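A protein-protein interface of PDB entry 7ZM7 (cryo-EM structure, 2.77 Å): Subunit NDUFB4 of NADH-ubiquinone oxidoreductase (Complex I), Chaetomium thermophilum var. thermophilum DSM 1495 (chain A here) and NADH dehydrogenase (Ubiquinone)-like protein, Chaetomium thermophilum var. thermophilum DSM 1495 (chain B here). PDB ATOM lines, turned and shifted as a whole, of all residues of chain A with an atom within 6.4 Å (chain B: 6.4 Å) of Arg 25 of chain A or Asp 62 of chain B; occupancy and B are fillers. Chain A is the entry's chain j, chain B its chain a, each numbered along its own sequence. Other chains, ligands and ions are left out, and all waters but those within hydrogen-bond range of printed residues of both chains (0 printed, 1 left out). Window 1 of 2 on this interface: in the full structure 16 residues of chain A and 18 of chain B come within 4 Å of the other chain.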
ATOM      1  N   SER A  20      28.251  -7.543 -36.178  1.00  0.00           N
ATOM      2  CA  SER A  20      26.838  -7.876 -36.193  1.00  0.00           C
ATOM      3  C   SER A  20      26.366  -8.337 -34.826  1.00  0.00           C
ATOM      4  O   SER A  20      25.172  -8.253 -34.520  1.00  0.00           O
ATOM      5  CB  SER A  20      26.576  -8.938 -37.246  1.00  0.00           C
ATOM      6  OG  SER A  20      27.198  -8.565 -38.457  1.00  0.00           O
ATOM      7  N   MET A  21      27.277  -8.831 -33.993  1.00  0.00           N
ATOM      8  CA  MET A  21      26.897  -9.146 -32.625  1.00  0.00           C
ATOM      9  C   MET A  21      26.641  -7.880 -31.824  1.00  0.00           C
ATOM     10  O   MET A  21      25.666  -7.801 -31.073  1.00  0.00           O
ATOM     11  CB  MET A  21      27.975  -9.987 -31.957  1.00  0.00           C
ATOM     12  CG  MET A  21      27.552 -10.541 -30.621  1.00  0.00           C
ATOM     13  SD  MET A  21      28.002  -9.471 -29.247  1.00  0.00           S
ATOM     14  CE  MET A  21      29.705  -9.936 -29.026  1.00  0.00           C
ATOM     15  N   ILE A  22      27.515  -6.887 -31.971  1.00  0.00           N
ATOM     16  CA  ILE A  22      27.448  -5.681 -31.157  1.00  0.00           C
ATOM     17  C   ILE A  22      26.236  -4.839 -31.533  1.00  0.00           C
ATOM     18  O   ILE A  22      25.514  -4.339 -30.665  1.00  0.00           O
ATOM     19  CB  ILE A  22      28.761  -4.896 -31.307  1.00  0.00           C
ATOM     20  CG1 ILE A  22      29.817  -5.476 -30.387  1.00  0.00           C
ATOM     21  CG2 ILE A  22      28.557  -3.460 -30.954  1.00  0.00           C
ATOM     22  CD1 ILE A  22      31.215  -5.038 -30.704  1.00  0.00           C
ATOM     23  N   SER A  23      25.980  -4.690 -32.829  1.00  0.00           N
ATOM     24  CA  SER A  23      24.871  -3.866 -33.283  1.00  0.00           C
ATOM     25  C   SER A  23      23.531  -4.422 -32.836  1.00  0.00           C
ATOM     26  O   SER A  23      22.574  -3.661 -32.658  1.00  0.00           O
ATOM     27  CB  SER A  23      24.904  -3.737 -34.800  1.00  0.00           C
ATOM     28  OG  SER A  23      26.037  -2.998 -35.210  1.00  0.00           O
ATOM     29  N   ASN A  24      23.437  -5.735 -32.665  1.00  0.00           N
ATOM     30  CA  ASN A  24      22.212  -6.393 -32.262  1.00  0.00           C
ATOM     31  C   ASN A  24      22.219  -6.797 -30.802  1.00  0.00           C
ATOM     32  O   ASN A  24      21.323  -7.514 -30.368  1.00  0.00           O
ATOM     33  CB  ASN A  24      21.979  -7.615 -33.138  1.00  0.00           C
ATOM     34  CG  ASN A  24      21.564  -7.254 -34.531  1.00  0.00           C
ATOM     35  OD1 ASN A  24      20.400  -6.969 -34.781  1.00  0.00           O
ATOM     36  ND2 ASN A  24      22.507  -7.270 -35.455  1.00  0.00           N
ATOM     37  N   ARG A  25      23.197  -6.330 -30.029  1.00  0.00           N
ATOM     38  CA  ARG A  25      23.419  -6.837 -28.676  1.00  0.00           C
ATOM     39  C   ARG A  25      22.228  -6.585 -27.759  1.00  0.00           C
ATOM     40  O   ARG A  25      21.842  -7.464 -26.988  1.00  0.00           O
ATOM     41  CB  ARG A  25      24.671  -6.191 -28.096  1.00  0.00           C
ATOM     42  CG  ARG A  25      25.039  -6.692 -26.741  1.00  0.00           C
ATOM     43  CD  ARG A  25      26.319  -6.086 -26.249  1.00  0.00           C
ATOM     44  NE  ARG A  25      26.592  -6.529 -24.889  1.00  0.00           N
ATOM     45  CZ  ARG A  25      27.235  -7.640 -24.569  1.00  0.00           C
ATOM     46  NH1 ARG A  25      27.727  -8.423 -25.506  1.00  0.00           N
ATOM     47  NH2 ARG A  25      27.415  -7.951 -23.301  1.00  0.00           N
ATOM     48  N   TYR A  26      21.642  -5.395 -27.828  1.00  0.00           N
ATOM     49  CA  TYR A  26      20.607  -4.977 -26.891  1.00  0.00           C
ATOM     50  C   TYR A  26      19.348  -5.835 -26.947  1.00  0.00           C
ATOM     51  O   TYR A  26      18.559  -5.811 -26.002  1.00  0.00           O
ATOM     52  CB  TYR A  26      20.250  -3.517 -27.167  1.00  0.00           C
ATOM     53  CG  TYR A  26      19.482  -3.361 -28.448  1.00  0.00           C
ATOM     54  CD1 TYR A  26      20.138  -3.376 -29.661  1.00  0.00           C
ATOM     55  CD2 TYR A  26      18.102  -3.261 -28.450  1.00  0.00           C
ATOM     56  CE1 TYR A  26      19.465  -3.272 -30.825  1.00  0.00           C
ATOM     57  CE2 TYR A  26      17.414  -3.159 -29.618  1.00  0.00           C
ATOM     58  CZ  TYR A  26      18.098  -3.173 -30.808  1.00  0.00           C
ATOM     59  OH  TYR A  26      17.427  -3.070 -31.996  1.00  0.00           O
ATOM     60  N   LYS A  27      19.124  -6.568 -28.029  1.00  0.00           N
ATOM     61  CA  LYS A  27      17.936  -7.397 -28.122  1.00  0.00           C
ATOM     62  C   LYS A  27      17.948  -8.525 -27.106  1.00  0.00           C
ATOM     63  O   LYS A  27      16.907  -9.138 -26.861  1.00  0.00           O
ATOM     64  CB  LYS A  27      17.822  -7.984 -29.514  1.00  0.00           C
ATOM     65  CG  LYS A  27      17.568  -6.983 -30.586  1.00  0.00           C
ATOM     66  CD  LYS A  27      17.308  -7.666 -31.884  1.00  0.00           C
ATOM     67  CE  LYS A  27      18.567  -8.229 -32.455  1.00  0.00           C
ATOM     68  NZ  LYS A  27      18.329  -8.810 -33.800  1.00  0.00           N
ATOM     69  N   TYR A  28      19.099  -8.800 -26.501  1.00  0.00           N
ATOM     70  CA  TYR A  28      19.252  -9.941 -25.622  1.00  0.00           C
ATOM     71  C   TYR A  28      19.546  -9.556 -24.184  1.00  0.00           C
ATOM     72  O   TYR A  28      19.797 -10.437 -23.368  1.00  0.00           O
ATOM     73  CB  TYR A  28      20.337 -10.879 -26.143  1.00  0.00           C
ATOM     74  CG  TYR A  28      20.245 -11.179 -27.605  1.00  0.00           C
ATOM     75  CD1 TYR A  28      20.659 -10.267 -28.555  1.00  0.00           C
ATOM     76  CD2 TYR A  28      19.666 -12.346 -28.042  1.00  0.00           C
ATOM     77  CE1 TYR A  28      20.558 -10.537 -29.870  1.00  0.00           C
ATOM     78  CE2 TYR A  28      19.554 -12.620 -29.360  1.00  0.00           C
ATOM     79  CZ  TYR A  28      19.999 -11.719 -30.271  1.00  0.00           C
ATOM     80  OH  TYR A  28      19.881 -12.003 -31.609  1.00  0.00           O
ATOM     81  N   PHE A  29      19.492  -8.279 -23.845  1.00  0.00           N
ATOM     82  CA  PHE A  29      19.703  -7.880 -22.465  1.00  0.00           C
ATOM     83  C   PHE A  29      18.541  -8.336 -21.593  1.00  0.00           C
ATOM     84  O   PHE A  29      17.372  -8.188 -21.954  1.00  0.00           O
ATOM     85  CB  PHE A  29      19.873  -6.367 -22.365  1.00  0.00           C
ATOM     86  CG  PHE A  29      20.028  -5.876 -20.963  1.00  0.00           C
ATOM     87  CD1 PHE A  29      21.257  -5.854 -20.360  1.00  0.00           C
ATOM     88  CD2 PHE A  29      18.931  -5.469 -20.238  1.00  0.00           C
ATOM     89  CE1 PHE A  29      21.390  -5.426 -19.081  1.00  0.00           C
ATOM     90  CE2 PHE A  29      19.064  -5.044 -18.953  1.00  0.00           C
ATOM     91  CZ  PHE A  29      20.298  -5.018 -18.377  1.00  0.00           C
ATOM     92  N   ARG A  30      18.899  -8.923 -20.448  1.00  0.00           N
ATOM     93  CA  ARG A  30      17.862  -9.401 -19.509  1.00  0.00           C
ATOM     94  C   ARG A  30      18.040  -8.756 -18.136  1.00  0.00           C
ATOM     95  O   ARG A  30      19.134  -8.258 -17.856  1.00  0.00           O
ATOM     96  CB  ARG A  30      17.965 -10.917 -19.339  1.00  0.00           C
ATOM     97  CG  ARG A  30      17.363 -11.768 -20.443  1.00  0.00           C
ATOM     98  CD  ARG A  30      17.553 -13.195 -19.963  1.00  0.00           C
ATOM     99  NE  ARG A  30      18.847 -13.315 -19.306  1.00  0.00           N
ATOM    100  CZ  ARG A  30      19.871 -14.029 -19.759  1.00  0.00           C
ATOM    101  NH1 ARG A  30      19.750 -14.731 -20.870  1.00  0.00           N
ATOM    102  NH2 ARG A  30      21.010 -14.049 -19.093  1.00  0.00           N
ATOM    103  N   ARG A  34      22.548  -9.632 -11.485  1.00  0.00           N
ATOM    104  CA  ARG A  34      23.807  -8.968 -11.788  1.00  0.00           C
ATOM    105  C   ARG A  34      23.576  -7.649 -12.511  1.00  0.00           C
ATOM    106  O   ARG A  34      24.232  -6.651 -12.206  1.00  0.00           O
ATOM    107  CB  ARG A  34      24.709  -9.881 -12.621  1.00  0.00           C
ATOM    108  CG  ARG A  34      26.077  -9.272 -12.914  1.00  0.00           C
ATOM    109  CD  ARG A  34      26.965 -10.196 -13.735  1.00  0.00           C
ATOM    110  NE  ARG A  34      26.421 -10.464 -15.062  1.00  0.00           N
ATOM    111  CZ  ARG A  34      26.579  -9.650 -16.101  1.00  0.00           C
ATOM    112  NH1 ARG A  34      27.275  -8.531 -15.964  1.00  0.00           N
ATOM    113  NH2 ARG A  34      26.052  -9.957 -17.281  1.00  0.00           N
ATOM    114  N   ASP B  57      19.150 -18.003 -19.447  1.00  0.00           N
ATOM    115  CA  ASP B  57      20.510 -18.053 -18.927  1.00  0.00           C
ATOM    116  C   ASP B  57      21.310 -19.208 -19.517  1.00  0.00           C
ATOM    117  O   ASP B  57      22.540 -19.128 -19.605  1.00  0.00           O
ATOM    118  CB  ASP B  57      20.476 -18.162 -17.404  1.00  0.00           C
ATOM    119  CG  ASP B  57      19.963 -16.903 -16.741  1.00  0.00           C
ATOM    120  OD1 ASP B  57      20.338 -15.800 -17.178  1.00  0.00           O
ATOM    121  OD2 ASP B  57      19.172 -17.017 -15.782  1.00  0.00           O
ATOM    122  N   ASP B  60      22.312 -18.326 -23.384  1.00  0.00           N
ATOM    123  CA  ASP B  60      22.985 -17.034 -23.527  1.00  0.00           C
ATOM    124  C   ASP B  60      23.379 -16.499 -22.162  1.00  0.00           C
ATOM    125  O   ASP B  60      22.627 -15.758 -21.519  1.00  0.00           O
ATOM    126  CB  ASP B  60      22.099 -16.033 -24.265  1.00  0.00           C
ATOM    127  CG  ASP B  60      22.877 -14.850 -24.781  1.00  0.00           C
ATOM    128  OD1 ASP B  60      24.113 -14.984 -24.923  1.00  0.00           O
ATOM    129  OD2 ASP B  60      22.260 -13.795 -25.048  1.00  0.00           O
ATOM    130  N   PRO B  61      24.551 -16.852 -21.686  1.00  0.00           N
ATOM    131  CA  PRO B  61      25.043 -16.257 -20.437  1.00  0.00           C
ATOM    132  C   PRO B  61      25.586 -14.842 -20.607  1.00  0.00           C
ATOM    133  O   PRO B  61      25.461 -14.016 -19.701  1.00  0.00           O
ATOM    134  CB  PRO B  61      26.141 -17.231 -19.994  1.00  0.00           C
ATOM    135  CG  PRO B  61      26.572 -17.921 -21.243  1.00  0.00           C
ATOM    136  CD  PRO B  61      25.403 -17.947 -22.175  1.00  0.00           C
ATOM    137  N   ASP B  62      26.182 -14.538 -21.757  1.00  0.00           N
ATOM    138  CA  ASP B  62      26.767 -13.219 -21.969  1.00  0.00           C
ATOM    139  C   ASP B  62      25.748 -12.168 -22.383  1.00  0.00           C
ATOM    140  O   ASP B  62      26.121 -11.005 -22.533  1.00  0.00           O
ATOM    141  CB  ASP B  62      27.870 -13.298 -23.021  1.00  0.00           C
ATOM    142  CG  ASP B  62      29.080 -14.072 -22.535  1.00  0.00           C
ATOM    143  OD1 ASP B  62      29.209 -14.263 -21.306  1.00  0.00           O
ATOM    144  OD2 ASP B  62      29.896 -14.495 -23.380  1.00  0.00           O
ATOM    145  N   MET B  63      24.487 -12.546 -22.562  1.00  0.00           N
ATOM    146  CA  MET B  63      23.426 -11.613 -22.934  1.00  0.00           C
ATOM    147  C   MET B  63      23.729 -10.941 -24.260  1.00  0.00           C
ATOM    148  O   MET B  63      23.346  -9.795 -24.492  1.00  0.00           O
ATOM    149  CB  MET B  63      23.198 -10.556 -21.854  1.00  0.00           C
ATOM    150  CG  MET B  63      22.433 -11.030 -20.691  1.00  0.00           C
ATOM    151  SD  MET B  63      22.075  -9.686 -19.595  1.00  0.00           S
ATOM    152  CE  MET B  63      21.368 -10.609 -18.270  1.00  0.00           C
ATOM    153  N   ASN B  64      24.438 -11.646 -25.133  1.00  0.00           N
ATOM    154  CA  ASN B  64      24.875 -11.064 -26.388  1.00  0.00           C
ATOM    155  C   ASN B  64      24.206 -11.671 -27.603  1.00  0.00           C
ATOM    156  O   ASN B  64      24.247 -11.058 -28.672  1.00  0.00           O
ATOM    157  CB  ASN B  64      26.402 -11.163 -26.533  1.00  0.00           C
ATOM    158  CG  ASN B  64      26.918 -12.577 -26.453  1.00  0.00           C
ATOM    159  OD1 ASN B  64      26.181 -13.538 -26.644  1.00  0.00           O
ATOM    160  ND2 ASN B  64      28.205 -12.713 -26.195  1.00  0.00           N
ATOM    161  N   GLY B  65      23.569 -12.822 -27.475  1.00  0.00           N
ATOM    162  CA  GLY B  65      22.834 -13.382 -28.584  1.00  0.00           C
ATOM    163  C   GLY B  65      23.181 -14.813 -28.888  1.00  0.00           C
ATOM    164  O   GLY B  65      22.925 -15.298 -29.990  1.00  0.00           O
ATOM    165  N   TYR B  67      26.299 -15.678 -28.883  1.00  0.00           N
ATOM    166  CA  TYR B  67      27.635 -15.564 -29.447  1.00  0.00           C
ATOM    167  C   TYR B  67      28.599 -16.471 -28.694  1.00  0.00           C
ATOM    168  O   TYR B  67      28.871 -16.260 -27.512  1.00  0.00           O
ATOM    169  CB  TYR B  67      28.093 -14.102 -29.401  1.00  0.00           C
ATOM    170  CG  TYR B  67      29.434 -13.816 -30.034  1.00  0.00           C
ATOM    171  CD1 TYR B  67      29.556 -13.632 -31.400  1.00  0.00           C
ATOM    172  CD2 TYR B  67      30.575 -13.706 -29.263  1.00  0.00           C
ATOM    173  CE1 TYR B  67      30.786 -13.363 -31.980  1.00  0.00           C
ATOM    174  CE2 TYR B  67      31.791 -13.432 -29.830  1.00  0.00           C
ATOM    175  CZ  TYR B  67      31.892 -13.266 -31.189  1.00  0.00           C
ATOM    176  OH  TYR B  67      33.111 -13.004 -31.750  1.00  0.00           O
ATOM    177  N   ILE B  68      29.101 -17.503 -29.364  1.00  0.00           N
ATOM    178  CA  ILE B  68      30.098 -18.363 -28.745  1.00  0.00           C
ATOM    179  C   ILE B  68      31.426 -17.623 -28.684  1.00  0.00           C
ATOM    180  O   ILE B  68      31.810 -16.910 -29.620  1.00  0.00           O
ATOM    181  CB  ILE B  68      30.205 -19.700 -29.494  1.00  0.00           C
ATOM    182  CG1 ILE B  68      31.009 -20.695 -28.664  1.00  0.00           C
ATOM    183  CG2 ILE B  68      30.801 -19.510 -30.880  1.00  0.00           C
ATOM    184  CD1 ILE B  68      30.331 -21.085 -27.388  1.00  0.00           C
ATOM    185  N   ASN B  69      32.123 -17.771 -27.569  1.00  0.00           N
ATOM    186  CA  ASN B  69      33.177 -16.853 -27.227  1.00  0.00           C
ATOM    187  C   ASN B  69      34.462 -17.593 -26.883  1.00  0.00           C
ATOM    188  O   ASN B  69      34.450 -18.491 -26.030  1.00  0.00           O
ATOM    189  CB  ASN B  69      32.737 -15.998 -26.053  1.00  0.00           C
ATOM    190  CG  ASN B  69      33.515 -14.735 -25.947  1.00  0.00           C
ATOM    191  OD1 ASN B  69      34.661 -14.756 -25.556  1.00  0.00           O
ATOM    192  ND2 ASN B  69      32.900 -13.618 -26.298  1.00  0.00           N
ATOM    193  N   GLU B  99      34.793 -11.127 -27.775  1.00  0.00           N
ATOM    194  CA  GLU B  99      34.093  -9.854 -27.915  1.00  0.00           C
ATOM    195  C   GLU B  99      34.900  -8.686 -27.373  1.00  0.00           C
ATOM    196  O   GLU B  99      34.574  -7.531 -27.656  1.00  0.00           O
ATOM    197  CB  GLU B  99      32.755  -9.897 -27.195  1.00  0.00           C
ATOM    198  CG  GLU B  99      32.871 -10.302 -25.756  1.00  0.00           C
ATOM    199  CD  GLU B  99      31.577 -10.836 -25.217  1.00  0.00           C
ATOM    200  OE1 GLU B  99      30.556 -10.734 -25.926  1.00  0.00           O
ATOM    201  OE2 GLU B  99      31.576 -11.362 -24.085  1.00  0.00           O
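Of the printed residues of chain B, Arg 25 of chain A touches Asp 62, Met 63, Asn 64 and Glu 99.
Of the printed residues of chain B, Tyr 28 of chain A touches Asp 60 (3.7 Å), Met 63 (3.6 Å), Asn 64 (3.7 Å) and Gly 65 (3.4 Å).
Printed residues of chain A within 4 Å of Gly 65 of chain B: Tyr 28 (3.4 Å).
Of the printed residues of chain A, Asp 57 of chain B touches Arg 30.
The nearest residue of chain B that does not touch Arg 25 of chain A is Gly 65 of chain B (5.7 Å).
The nearest residue of chain A that does not touch Asp 62 of chain B is Arg 34 of chain A (5.4 Å).
The backbone NH (N) of Arg 30 of chain A is in hydrogen-bond range of the side-chain sulfur (SD) of Met 63 of chain B, 3.4 Å away.
OD1 of Asp 57 of chain B lies within salt-bridge range of NH2 of Arg 30 of chain A, at 2.7 Å.
The backbone carbonyl oxygen (O) of Asp 60 of chain B lies within hydrogen-bond range of the guanidinium group (NH1) of Arg 30 of chain A (3.1 Å).
OE1 of Glu 99 of chain B is in salt-bridge range of NH1 of Arg 25 of chain A (3.7 Å).
NH2 of Arg 25 of chain A sits at hydrogen-bond distance from O of Asp 62 of chain B (3.4 Å).
OD2 of Asp 60 of chain B is in hydrogen-bond range of N of Gly 65 of chain B.
The side-chain amide nitrogen (ND2) of Asn 69 of chain B sits close to the side-chain carboxylate (OE2) of Glu 99 of chain B, 3.4 Å away.
The side-chain carboxylate (OD1) of Asp 60 of chain B sits at hydrogen-bond distance from the backbone NH (N) of Met 63 of chain B, 3.4 Å away.
ND2 of Asn 64 of chain B is in hydrogen-bond range of OE1 of Glu 99 of chain B (3.1 Å).
The side-chain amide oxygen (OD1) of Asn 64 of chain B lies within hydrogen-bond range of the backbone NH (N) of Tyr 67 of chain B, 3.1 Å away.
OD1 of Asp 60 of chain B sits close to OD1 of Asn 64 of chain B.
Of the 11 printed residues of chain B, 8 touch a printed residue of chain A.
Printed residues of chain B that touch a printed residue of chain A: Asp 57, Asp 60, Asp 62, Met 63, Asn 64, Gly 65, Tyr 67 and Glu 99.
Hydrophobic or aromatic side chains of chain B that line the printed part of chain A: Met 63 and Tyr 67.
Hydrophobic or aromatic side chains of chain A within 4 Å of the printed part of chain B: Met 21, Tyr 28 and Phe 29.
Among the printed residues, Asp or Glu carboxylates within 4 Å of a Lys or Arg side-chain nitrogen of the other chain: Arg 25 of chain A with Glu 99 of chain B (3.7 Å) and Arg 30 of chain A with Asp 57 of chain B (2.7 Å).
Among the printed residues, merely in contact across the chains: Arg 25 of chain A with Asn 64 of chain B (3.2 Å), Met 21 of chain A with Glu 99 of chain B (3.3 Å), Tyr 28 of chain A with Gly 65 of chain B (3.4 Å), Met 21 of chain A with Asn 64 of chain B (3.6 Å), Tyr 28 of chain A with Met 63 of chain B (3.6 Å), Tyr 28 of chain A with Asp 60 of chain B (3.7 Å), Tyr 28 of chain A with Asn 64 of chain B (3.7 Å), Arg 25 of chain A with Met 63 of chain B (3.7 Å), Met 21 of chain A with Tyr 67 of chain B (3.8 Å) and Phe 29 of chain A with Met 63 of chain B (3.99 Å).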
